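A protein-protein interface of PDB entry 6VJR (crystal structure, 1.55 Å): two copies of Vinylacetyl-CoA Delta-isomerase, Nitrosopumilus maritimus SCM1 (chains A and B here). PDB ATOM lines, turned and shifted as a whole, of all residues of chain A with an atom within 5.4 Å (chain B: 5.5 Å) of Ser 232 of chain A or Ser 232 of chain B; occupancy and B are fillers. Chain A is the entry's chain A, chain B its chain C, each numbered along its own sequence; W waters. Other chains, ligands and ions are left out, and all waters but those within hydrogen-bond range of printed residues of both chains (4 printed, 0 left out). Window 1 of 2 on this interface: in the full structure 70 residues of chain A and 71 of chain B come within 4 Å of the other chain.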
ATOM      1  N   ARG A 230     -19.129 -10.699  -4.808  1.00  0.00           N
ATOM      2  CA  ARG A 230     -18.187 -11.097  -5.836  1.00  0.00           C
ATOM      3  C   ARG A 230     -18.926 -11.857  -6.926  1.00  0.00           C
ATOM      4  O   ARG A 230     -20.030 -12.345  -6.714  1.00  0.00           O
ATOM      5  CB  ARG A 230     -17.096 -11.996  -5.272  1.00  0.00           C
ATOM      6  CG  ARG A 230     -16.106 -11.298  -4.361  1.00  0.00           C
ATOM      7  CD  ARG A 230     -14.790 -12.020  -4.315  1.00  0.00           C
ATOM      8  NE  ARG A 230     -14.040 -11.788  -5.554  1.00  0.00           N
ATOM      9  CZ  ARG A 230     -12.714 -11.777  -5.624  1.00  0.00           C
ATOM     10  NH1 ARG A 230     -11.966 -12.166  -4.585  1.00  0.00           N
ATOM     11  NH2 ARG A 230     -12.133 -11.472  -6.774  1.00  0.00           N
ATOM     12  N   GLN A 231     -18.301 -11.979  -8.080  1.00  0.00           N
ATOM     13  CA  GLN A 231     -18.777 -12.827  -9.150  1.00  0.00           C
ATOM     14  C   GLN A 231     -17.556 -13.571  -9.706  1.00  0.00           C
ATOM     15  O   GLN A 231     -16.435 -13.026  -9.658  1.00  0.00           O
ATOM     16  CB  GLN A 231     -19.443 -12.049 -10.280  1.00  0.00           C
ATOM     17  CG  GLN A 231     -20.676 -11.286  -9.838  1.00  0.00           C
ATOM     18  CD  GLN A 231     -21.425 -10.673 -10.995  1.00  0.00           C
ATOM     19  OE1 GLN A 231     -20.826 -10.265 -11.993  1.00  0.00           O
ATOM     20  NE2 GLN A 231     -22.748 -10.644 -10.894  1.00  0.00           N
ATOM     21  N   SER A 232     -17.808 -14.754 -10.273  1.00  0.00           N
ATOM     22  CA  SER A 232     -16.801 -15.458 -11.053  1.00  0.00           C
ATOM     23  C   SER A 232     -16.175 -14.516 -12.094  1.00  0.00           C
ATOM     24  O   SER A 232     -16.895 -13.924 -12.862  1.00  0.00           O
ATOM     25  CB  SER A 232     -17.354 -16.689 -11.697  1.00  0.00           C
ATOM     26  OG  SER A 232     -16.302 -17.317 -12.415  1.00  0.00           O
ATOM     27  N   CYS A 233     -14.847 -14.342 -12.077  1.00  0.00           N
ATOM     28  CA  CYS A 233     -14.146 -13.512 -13.055  1.00  0.00           C
ATOM     29  C   CYS A 233     -14.450 -12.020 -12.907  1.00  0.00           C
ATOM     30  O   CYS A 233     -14.144 -11.237 -13.833  1.00  0.00           O
ATOM     31  CB  CYS A 233     -14.381 -13.963 -14.512  1.00  0.00           C
ATOM     32  SG  CYS A 233     -13.822 -15.635 -14.837  1.00  0.00           S
ATOM     33  N   ASP A 234     -14.961 -11.602 -11.736  1.00  0.00           N
ATOM     34  CA  ASP A 234     -15.373 -10.213 -11.517  1.00  0.00           C
ATOM     35  C   ASP A 234     -14.259  -9.227 -11.909  1.00  0.00           C
ATOM     36  O   ASP A 234     -14.502  -8.237 -12.601  1.00  0.00           O
ATOM     37  CB  ASP A 234     -15.829 -10.000 -10.082  1.00  0.00           C
ATOM     38  CG  ASP A 234     -14.984 -10.579  -8.943  1.00  0.00           C
ATOM     39  OD1 ASP A 234     -13.808 -11.000  -9.183  1.00  0.00           O
ATOM     40  OD2 ASP A 234     -15.526 -10.690  -7.819  1.00  0.00           O
ATOM     41  N   ARG A 236     -11.833  -9.231 -13.915  1.00  0.00           N
ATOM     42  CA  ARG A 236     -11.403  -8.987 -15.274  1.00  0.00           C
ATOM     43  C   ARG A 236     -11.876  -7.615 -15.741  1.00  0.00           C
ATOM     44  O   ARG A 236     -11.247  -6.987 -16.619  1.00  0.00           O
ATOM     45  CB  ARG A 236     -11.910 -10.058 -16.229  1.00  0.00           C
ATOM     46  CG  ARG A 236     -11.229 -11.389 -15.947  1.00  0.00           C
ATOM     47  CD  ARG A 236     -11.530 -12.393 -16.988  1.00  0.00           C
ATOM     48  NE  ARG A 236     -11.017 -13.735 -16.703  1.00  0.00           N
ATOM     49  CZ  ARG A 236     -11.109 -14.765 -17.512  1.00  0.00           C
ATOM     50  NH1 ARG A 236     -11.620 -14.617 -18.698  1.00  0.00           N
ATOM     51  NH2 ARG A 236     -10.676 -15.986 -17.147  1.00  0.00           N
ATOM     52  N   GLU A 429     -16.981 -18.426 -22.507  1.00  0.00           N
ATOM     53  CA  GLU A 429     -16.451 -18.565 -21.153  1.00  0.00           C
ATOM     54  C   GLU A 429     -17.231 -17.699 -20.155  1.00  0.00           C
ATOM     55  O   GLU A 429     -17.617 -18.128 -19.078  1.00  0.00           O
ATOM     56  CB  GLU A 429     -14.961 -18.223 -21.154  1.00  0.00           C
ATOM     57  CG  GLU A 429     -14.267 -18.471 -19.824  1.00  0.00           C
ATOM     58  CD  GLU A 429     -12.921 -17.744 -19.610  1.00  0.00           C
ATOM     59  OE1 GLU A 429     -12.653 -16.746 -20.334  1.00  0.00           O
ATOM     60  OE2 GLU A 429     -12.117 -18.160 -18.732  1.00  0.00           O
ATOM     61  N   LEU A 433     -18.889 -20.005 -17.370  1.00  0.00           N
ATOM     62  CA  LEU A 433     -18.046 -20.051 -16.186  1.00  0.00           C
ATOM     63  C   LEU A 433     -17.913 -18.700 -15.477  1.00  0.00           C
ATOM     64  O   LEU A 433     -17.717 -18.657 -14.262  1.00  0.00           O
ATOM     65  CB  LEU A 433     -16.659 -20.587 -16.523  1.00  0.00           C
ATOM     66  CG  LEU A 433     -16.609 -22.025 -17.021  1.00  0.00           C
ATOM     67  CD1 LEU A 433     -15.219 -22.404 -17.498  1.00  0.00           C
ATOM     68  CD2 LEU A 433     -17.083 -22.911 -15.942  1.00  0.00           C
ATOM     69  N   GLY A 434     -17.954 -17.607 -16.217  1.00  0.00           N
ATOM     70  CA  GLY A 434     -17.570 -16.304 -15.727  1.00  0.00           C
ATOM     71  C   GLY A 434     -18.726 -15.472 -15.217  1.00  0.00           C
ATOM     72  O   GLY A 434     -19.709 -15.992 -14.667  1.00  0.00           O
ATOM     73  N   ARG A 435     -18.595 -14.147 -15.441  1.00  0.00           N
ATOM     74  CA  ARG A 435     -19.417 -13.228 -14.678  1.00  0.00           C
ATOM     75  C   ARG A 435     -20.892 -13.401 -15.031  1.00  0.00           C
ATOM     76  O   ARG A 435     -21.765 -13.226 -14.170  1.00  0.00           O
ATOM     77  CB  ARG A 435     -19.034 -11.776 -14.992  1.00  0.00           C
ATOM     78  CG  ARG A 435     -17.849 -11.196 -14.261  1.00  0.00           C
ATOM     79  CD  ARG A 435     -17.804  -9.693 -14.376  1.00  0.00           C
ATOM     80  NE  ARG A 435     -18.572  -9.118 -13.264  1.00  0.00           N
ATOM     81  CZ  ARG A 435     -18.656  -7.846 -12.965  1.00  0.00           C
ATOM     82  NH1 ARG A 435     -19.323  -7.481 -11.871  1.00  0.00           N
ATOM     83  NH2 ARG A 435     -18.062  -6.968 -13.745  1.00  0.00           N
ATOM     84  N   VAL A 438     -23.087 -16.360 -13.476  1.00  0.00           N
ATOM     85  CA  VAL A 438     -23.786 -16.116 -12.227  1.00  0.00           C
ATOM     86  C   VAL A 438     -25.280 -15.980 -12.474  1.00  0.00           C
ATOM     87  O   VAL A 438     -26.082 -16.602 -11.801  1.00  0.00           O
ATOM     88  CB  VAL A 438     -23.233 -14.883 -11.510  1.00  0.00           C
ATOM     89  CG1 VAL A 438     -24.126 -14.415 -10.358  1.00  0.00           C
ATOM     90  CG2 VAL A 438     -21.826 -15.168 -11.071  1.00  0.00           C
ATOM     91  N   ARG B 230      -5.184 -18.671 -19.429  1.00  0.00           N
ATOM     92  CA  ARG B 230      -6.022 -18.159 -18.357  1.00  0.00           C
ATOM     93  C   ARG B 230      -6.941 -19.261 -17.817  1.00  0.00           C
ATOM     94  O   ARG B 230      -7.249 -20.242 -18.468  1.00  0.00           O
ATOM     95  CB  ARG B 230      -6.854 -16.943 -18.772  1.00  0.00           C
ATOM     96  CG  ARG B 230      -6.055 -15.705 -19.113  1.00  0.00           C
ATOM     97  CD  ARG B 230      -6.891 -14.453 -18.992  1.00  0.00           C
ATOM     98  NE  ARG B 230      -7.174 -14.125 -17.593  1.00  0.00           N
ATOM     99  CZ  ARG B 230      -7.476 -12.907 -17.141  1.00  0.00           C
ATOM    100  NH1 ARG B 230      -7.623 -11.898 -17.995  1.00  0.00           N
ATOM    101  NH2 ARG B 230      -7.593 -12.702 -15.851  1.00  0.00           N
ATOM    102  N   GLN B 231      -7.448 -19.040 -16.625  1.00  0.00           N
ATOM    103  CA  GLN B 231      -8.528 -19.843 -16.080  1.00  0.00           C
ATOM    104  C   GLN B 231      -9.569 -18.916 -15.461  1.00  0.00           C
ATOM    105  O   GLN B 231      -9.226 -17.827 -15.007  1.00  0.00           O
ATOM    106  CB  GLN B 231      -8.068 -20.815 -15.005  1.00  0.00           C
ATOM    107  CG  GLN B 231      -7.021 -21.782 -15.534  1.00  0.00           C
ATOM    108  CD  GLN B 231      -6.659 -22.832 -14.515  1.00  0.00           C
ATOM    109  OE1 GLN B 231      -6.659 -22.578 -13.309  1.00  0.00           O
ATOM    110  NE2 GLN B 231      -6.332 -24.029 -14.994  1.00  0.00           N
ATOM    111  N   SER B 232     -10.823 -19.390 -15.425  1.00  0.00           N
ATOM    112  CA  SER B 232     -11.845 -18.697 -14.670  1.00  0.00           C
ATOM    113  C   SER B 232     -11.370 -18.441 -13.244  1.00  0.00           C
ATOM    114  O   SER B 232     -10.924 -19.361 -12.572  1.00  0.00           O
ATOM    115  CB  SER B 232     -13.123 -19.489 -14.691  1.00  0.00           C
ATOM    116  OG  SER B 232     -14.090 -18.825 -13.924  1.00  0.00           O
ATOM    117  N   CYS B 233     -11.437 -17.195 -12.790  1.00  0.00           N
ATOM    118  CA  CYS B 233     -11.038 -16.819 -11.438  1.00  0.00           C
ATOM    119  C   CYS B 233      -9.541 -16.947 -11.179  1.00  0.00           C
ATOM    120  O   CYS B 233      -9.115 -16.912 -10.008  1.00  0.00           O
ATOM    121  CB  CYS B 233     -11.843 -17.514 -10.326  1.00  0.00           C
ATOM    122  SG  CYS B 233     -13.611 -17.199 -10.439  1.00  0.00           S
ATOM    123  N   ASP B 234      -8.735 -17.028 -12.250  1.00  0.00           N
ATOM    124  CA  ASP B 234      -7.291 -17.231 -12.118  1.00  0.00           C
ATOM    125  C   ASP B 234      -6.621 -16.273 -11.134  1.00  0.00           C
ATOM    126  O   ASP B 234      -5.829 -16.678 -10.245  1.00  0.00           O
ATOM    127  CB  ASP B 234      -6.585 -17.173 -13.469  1.00  0.00           C
ATOM    128  CG  ASP B 234      -6.954 -16.070 -14.460  1.00  0.00           C
ATOM    129  OD1 ASP B 234      -7.579 -15.067 -14.042  1.00  0.00           O
ATOM    130  OD2 ASP B 234      -6.622 -16.232 -15.656  1.00  0.00           O
ATOM    131  N   ARG B 236      -7.604 -14.637  -8.645  1.00  0.00           N
ATOM    132  CA  ARG B 236      -7.861 -14.685  -7.205  1.00  0.00           C
ATOM    133  C   ARG B 236      -6.639 -15.230  -6.457  1.00  0.00           C
ATOM    134  O   ARG B 236      -6.389 -14.866  -5.313  1.00  0.00           O
ATOM    135  CB  ARG B 236      -9.118 -15.457  -6.803  1.00  0.00           C
ATOM    136  CG  ARG B 236     -10.389 -14.842  -7.372  1.00  0.00           C
ATOM    137  CD  ARG B 236     -11.562 -15.478  -6.731  1.00  0.00           C
ATOM    138  NE  ARG B 236     -12.812 -15.010  -7.311  1.00  0.00           N
ATOM    139  CZ  ARG B 236     -13.990 -15.450  -6.942  1.00  0.00           C
ATOM    140  NH1 ARG B 236     -14.101 -16.322  -5.961  1.00  0.00           N
ATOM    141  NH2 ARG B 236     -15.066 -15.022  -7.544  1.00  0.00           N
ATOM    142  N   GLU B 429     -18.007 -22.778  -5.336  1.00  0.00           N
ATOM    143  CA  GLU B 429     -17.816 -21.843  -6.434  1.00  0.00           C
ATOM    144  C   GLU B 429     -16.588 -22.222  -7.275  1.00  0.00           C
ATOM    145  O   GLU B 429     -16.644 -22.260  -8.498  1.00  0.00           O
ATOM    146  CB  GLU B 429     -17.691 -20.403  -5.923  1.00  0.00           C
ATOM    147  CG  GLU B 429     -17.666 -19.344  -7.036  1.00  0.00           C
ATOM    148  CD  GLU B 429     -17.108 -17.990  -6.596  1.00  0.00           C
ATOM    149  OE1 GLU B 429     -16.404 -17.881  -5.561  1.00  0.00           O
ATOM    150  OE2 GLU B 429     -17.394 -16.973  -7.257  1.00  0.00           O
ATOM    151  N   LEU B 433     -17.691 -23.036 -11.054  1.00  0.00           N
ATOM    152  CA  LEU B 433     -17.540 -21.859 -11.908  1.00  0.00           C
ATOM    153  C   LEU B 433     -16.094 -21.404 -12.041  1.00  0.00           C
ATOM    154  O   LEU B 433     -15.744 -20.839 -13.086  1.00  0.00           O
ATOM    155  CB  LEU B 433     -18.364 -20.663 -11.438  1.00  0.00           C
ATOM    156  CG  LEU B 433     -19.862 -20.881 -11.374  1.00  0.00           C
ATOM    157  CD1 LEU B 433     -20.557 -19.772 -10.638  1.00  0.00           C
ATOM    158  CD2 LEU B 433     -20.395 -20.994 -12.771  1.00  0.00           C
ATOM    159  N   GLY B 434     -15.271 -21.606 -11.031  1.00  0.00           N
ATOM    160  CA  GLY B 434     -13.947 -20.998 -10.964  1.00  0.00           C
ATOM    161  C   GLY B 434     -12.816 -21.922 -11.428  1.00  0.00           C
ATOM    162  O   GLY B 434     -12.972 -22.696 -12.381  1.00  0.00           O
ATOM    163  N   ARG B 435     -11.633 -21.745 -10.848  1.00  0.00           N
ATOM    164  CA  ARG B 435     -10.438 -22.302 -11.473  1.00  0.00           C
ATOM    165  C   ARG B 435     -10.508 -23.826 -11.608  1.00  0.00           C
ATOM    166  O   ARG B 435      -9.968 -24.363 -12.591  1.00  0.00           O
ATOM    167  CB  ARG B 435      -9.143 -22.014 -10.694  1.00  0.00           C
ATOM    168  CG  ARG B 435      -8.617 -20.615 -10.702  1.00  0.00           C
ATOM    169  CD  ARG B 435      -7.286 -20.536 -10.075  1.00  0.00           C
ATOM    170  NE  ARG B 435      -6.308 -20.804 -11.137  1.00  0.00           N
ATOM    171  CZ  ARG B 435      -4.972 -20.662 -11.034  1.00  0.00           C
ATOM    172  NH1 ARG B 435      -4.211 -20.864 -12.084  1.00  0.00           N
ATOM    173  NH2 ARG B 435      -4.417 -20.290  -9.904  1.00  0.00           N
ATOM    174  N   VAL B 438     -12.459 -25.567 -14.552  1.00  0.00           N
ATOM    175  CA  VAL B 438     -11.786 -25.761 -15.818  1.00  0.00           C
ATOM    176  C   VAL B 438     -11.521 -27.250 -15.985  1.00  0.00           C
ATOM    177  O   VAL B 438     -11.801 -27.823 -17.032  1.00  0.00           O
ATOM    178  CB  VAL B 438     -10.496 -24.937 -15.896  1.00  0.00           C
ATOM    179  CG1 VAL B 438      -9.620 -25.368 -17.057  1.00  0.00           C
ATOM    180  CG2 VAL B 438     -10.857 -23.461 -15.974  1.00  0.00           C
HETATM  181  O   HOH W   1     -10.259 -14.384 -13.984  1.00  0.00           O
HETATM  182  O   HOH W   2     -11.377 -20.660 -18.095  1.00  0.00           O
HETATM  183  O   HOH W   3     -19.681 -16.082  -8.472  1.00  0.00           O
HETATM  184  O   HOH W   4     -12.734 -13.436  -9.786  1.00  0.00           O
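The backbone carbonyl oxygen (O) of Gln 231 of chain A is in hydrogen-bond range of the guanidinium group (NH2) of Arg 236 of chain B (3.2 Å). The side-chain hydroxyl of Ser 232 of chain A lies within hydrogen-bond range of the side-chain hydroxyl of Ser 232 of chain B (3.1 Å). The side-chain sulfur (SG) of Cys 233 of chain B sits at hydrogen-bond distance from the side-chain hydroxyl (OG) of Ser 232 of chain A. The side-chain hydroxyl (OG) of Ser 232 of chain B lies within hydrogen-bond range of the side-chain sulfur (SG) of Cys 233 of chain A (3.3 Å). N of Cys 233 of chain B lies within hydrogen-bond range of SG of Cys 233 of chain A (3.5 Å). The guanidinium group of Arg 236 of chain A sits at hydrogen-bond distance from the backbone carbonyl oxygen of Gln 231 of chain B (3.2 Å). O of Leu 433 of chain B sits close to O of Leu 433 of chain A (3.2 Å).
The guanidinium group (NE) of Arg 230 of chain A lies within salt-bridge range of the side-chain carboxylate (OD2) of Asp 234 of chain A, 2.9 Å away. The guanidinium group (NH1) of Arg 236 of chain A is in salt-bridge range of the side-chain carboxylate (OE1) of Glu 429 of chain A, 2.9 Å away. The side-chain carboxylate (OD2) of Asp 234 of chain B lies within hydrogen-bond range of the backbone NH (N) of Gln 231 of chain B (3.1 Å). NE of Arg 435 of chain B sits at hydrogen-bond distance from OE1 of Gln 231 of chain B, 2.8 Å away. The side-chain hydroxyl of Ser 232 of chain B sits at hydrogen-bond distance from the backbone carbonyl oxygen of Leu 433 of chain B (2.7 Å). The backbone carbonyl oxygen of Ser 232 of chain B is in hydrogen-bond range of the backbone NH of Arg 435 of chain B.
Among the printed residues, merely in contact across the chains: Ser 232 of chain A with Leu 433 of chain B, Arg 230 of chain A with Arg 236 of chain B, Leu 433 of chain A with Ser 232 of chain B, Arg 236 of chain A with Arg 230 of chain B, Glu 429 of chain A with Ser 232 of chain B, Ser 232 of chain A with Glu 429 of chain B, Arg 236 of chain A with Ser 232 of chain B and Ser 232 of chain A with Arg 236 of chain B.
Ser 232 of chain A touches just these residues of chain B: Ser 232 (3.1 Å), Cys 233 (3.3 Å), Arg 236 (3.9 Å), Glu 429 (3.8 Å) and Leu 433 (3.6 Å). Printed residues of chain B within 4 Å of Cys 233 of chain A: Ser 232 (3.3 Å) and Cys 233 (3.5 Å). Printed residues of chain A within 4 Å of Gln 231 of chain B: Arg 236. Ser 232 of chain B touches just these residues of chain A: Ser 232 (3.1 Å), Cys 233 (3.3 Å), Arg 236 (3.8 Å), Glu 429 (3.8 Å) and Leu 433 (3.6 Å). Printed residues of chain A within 4 Å of Cys 233 of chain B: Ser 232 and Cys 233. Asp 234 of chain B touches none of the printed residues of chain A. Of the printed residues of chain A, Leu 433 of chain B touches Ser 232 and Leu 433. Arg 435 of chain B touches none of the printed residues of chain A. The nearest residue of chain A that does not touch Ser 232 of chain B is Gly 434 of chain A (4.7 Å). The nearest printed residue of chain B that does not touch Glu 429 of chain A is Gln 231 of chain B (4.2 Å).
Hydrophobic or aromatic side chains of chain B that line the printed part of chain A: Leu 433. Along chain B the printed residues that touch a printed residue of chain A span positions 230 to 433. Among the printed residues, 15 pairs touch across the chains.
Arg 230 of chain A touches Arg 236 of chain B, and with the chains exchanged Arg 236 of chain A touches Arg 230 of chain B. Ser 232 of chain A touches Cys 233 of chain B, and with the chains exchanged Cys 233 of chain A touches Ser 232 of chain B. Ser 232 of chain A touches Glu 429 of chain B, and with the chains exchanged Glu 429 of chain A touches Ser 232 of chain B. Ser 232 of chain A touches Leu 433 of chain B, and with the chains exchanged Leu 433 of chain A touches Ser 232 of chain B. Of the 15 pairs that touch across the chains among the printed residues, 15 have their exchanged pair printed and touching as well.
Water W2 lies within hydrogen-bond range of the side-chain carboxylate of Glu 429 of chain A (2.7 Å) and the backbone NH of Ser 232 of chain B (3.0 Å). Water W4 lies within hydrogen-bond range of OD1 of Asp 234 of chain A, NE of Arg 236 of chain B and N of Cys 233 of chain A. Water W3 lies within hydrogen-bond range of OE2 of Glu 429 of chain B (2.7 Å) and N of Ser 232 of chain A (2.9 Å). Water W1 lies within hydrogen-bond range of the side-chain carboxylate (OD1) of Asp 234 of chain B (2.8 Å), the guanidinium group (NE) of Arg 236 of chain A (2.9 Å) and the backbone NH (N) of Cys 233 of chain B (3.3 Å).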
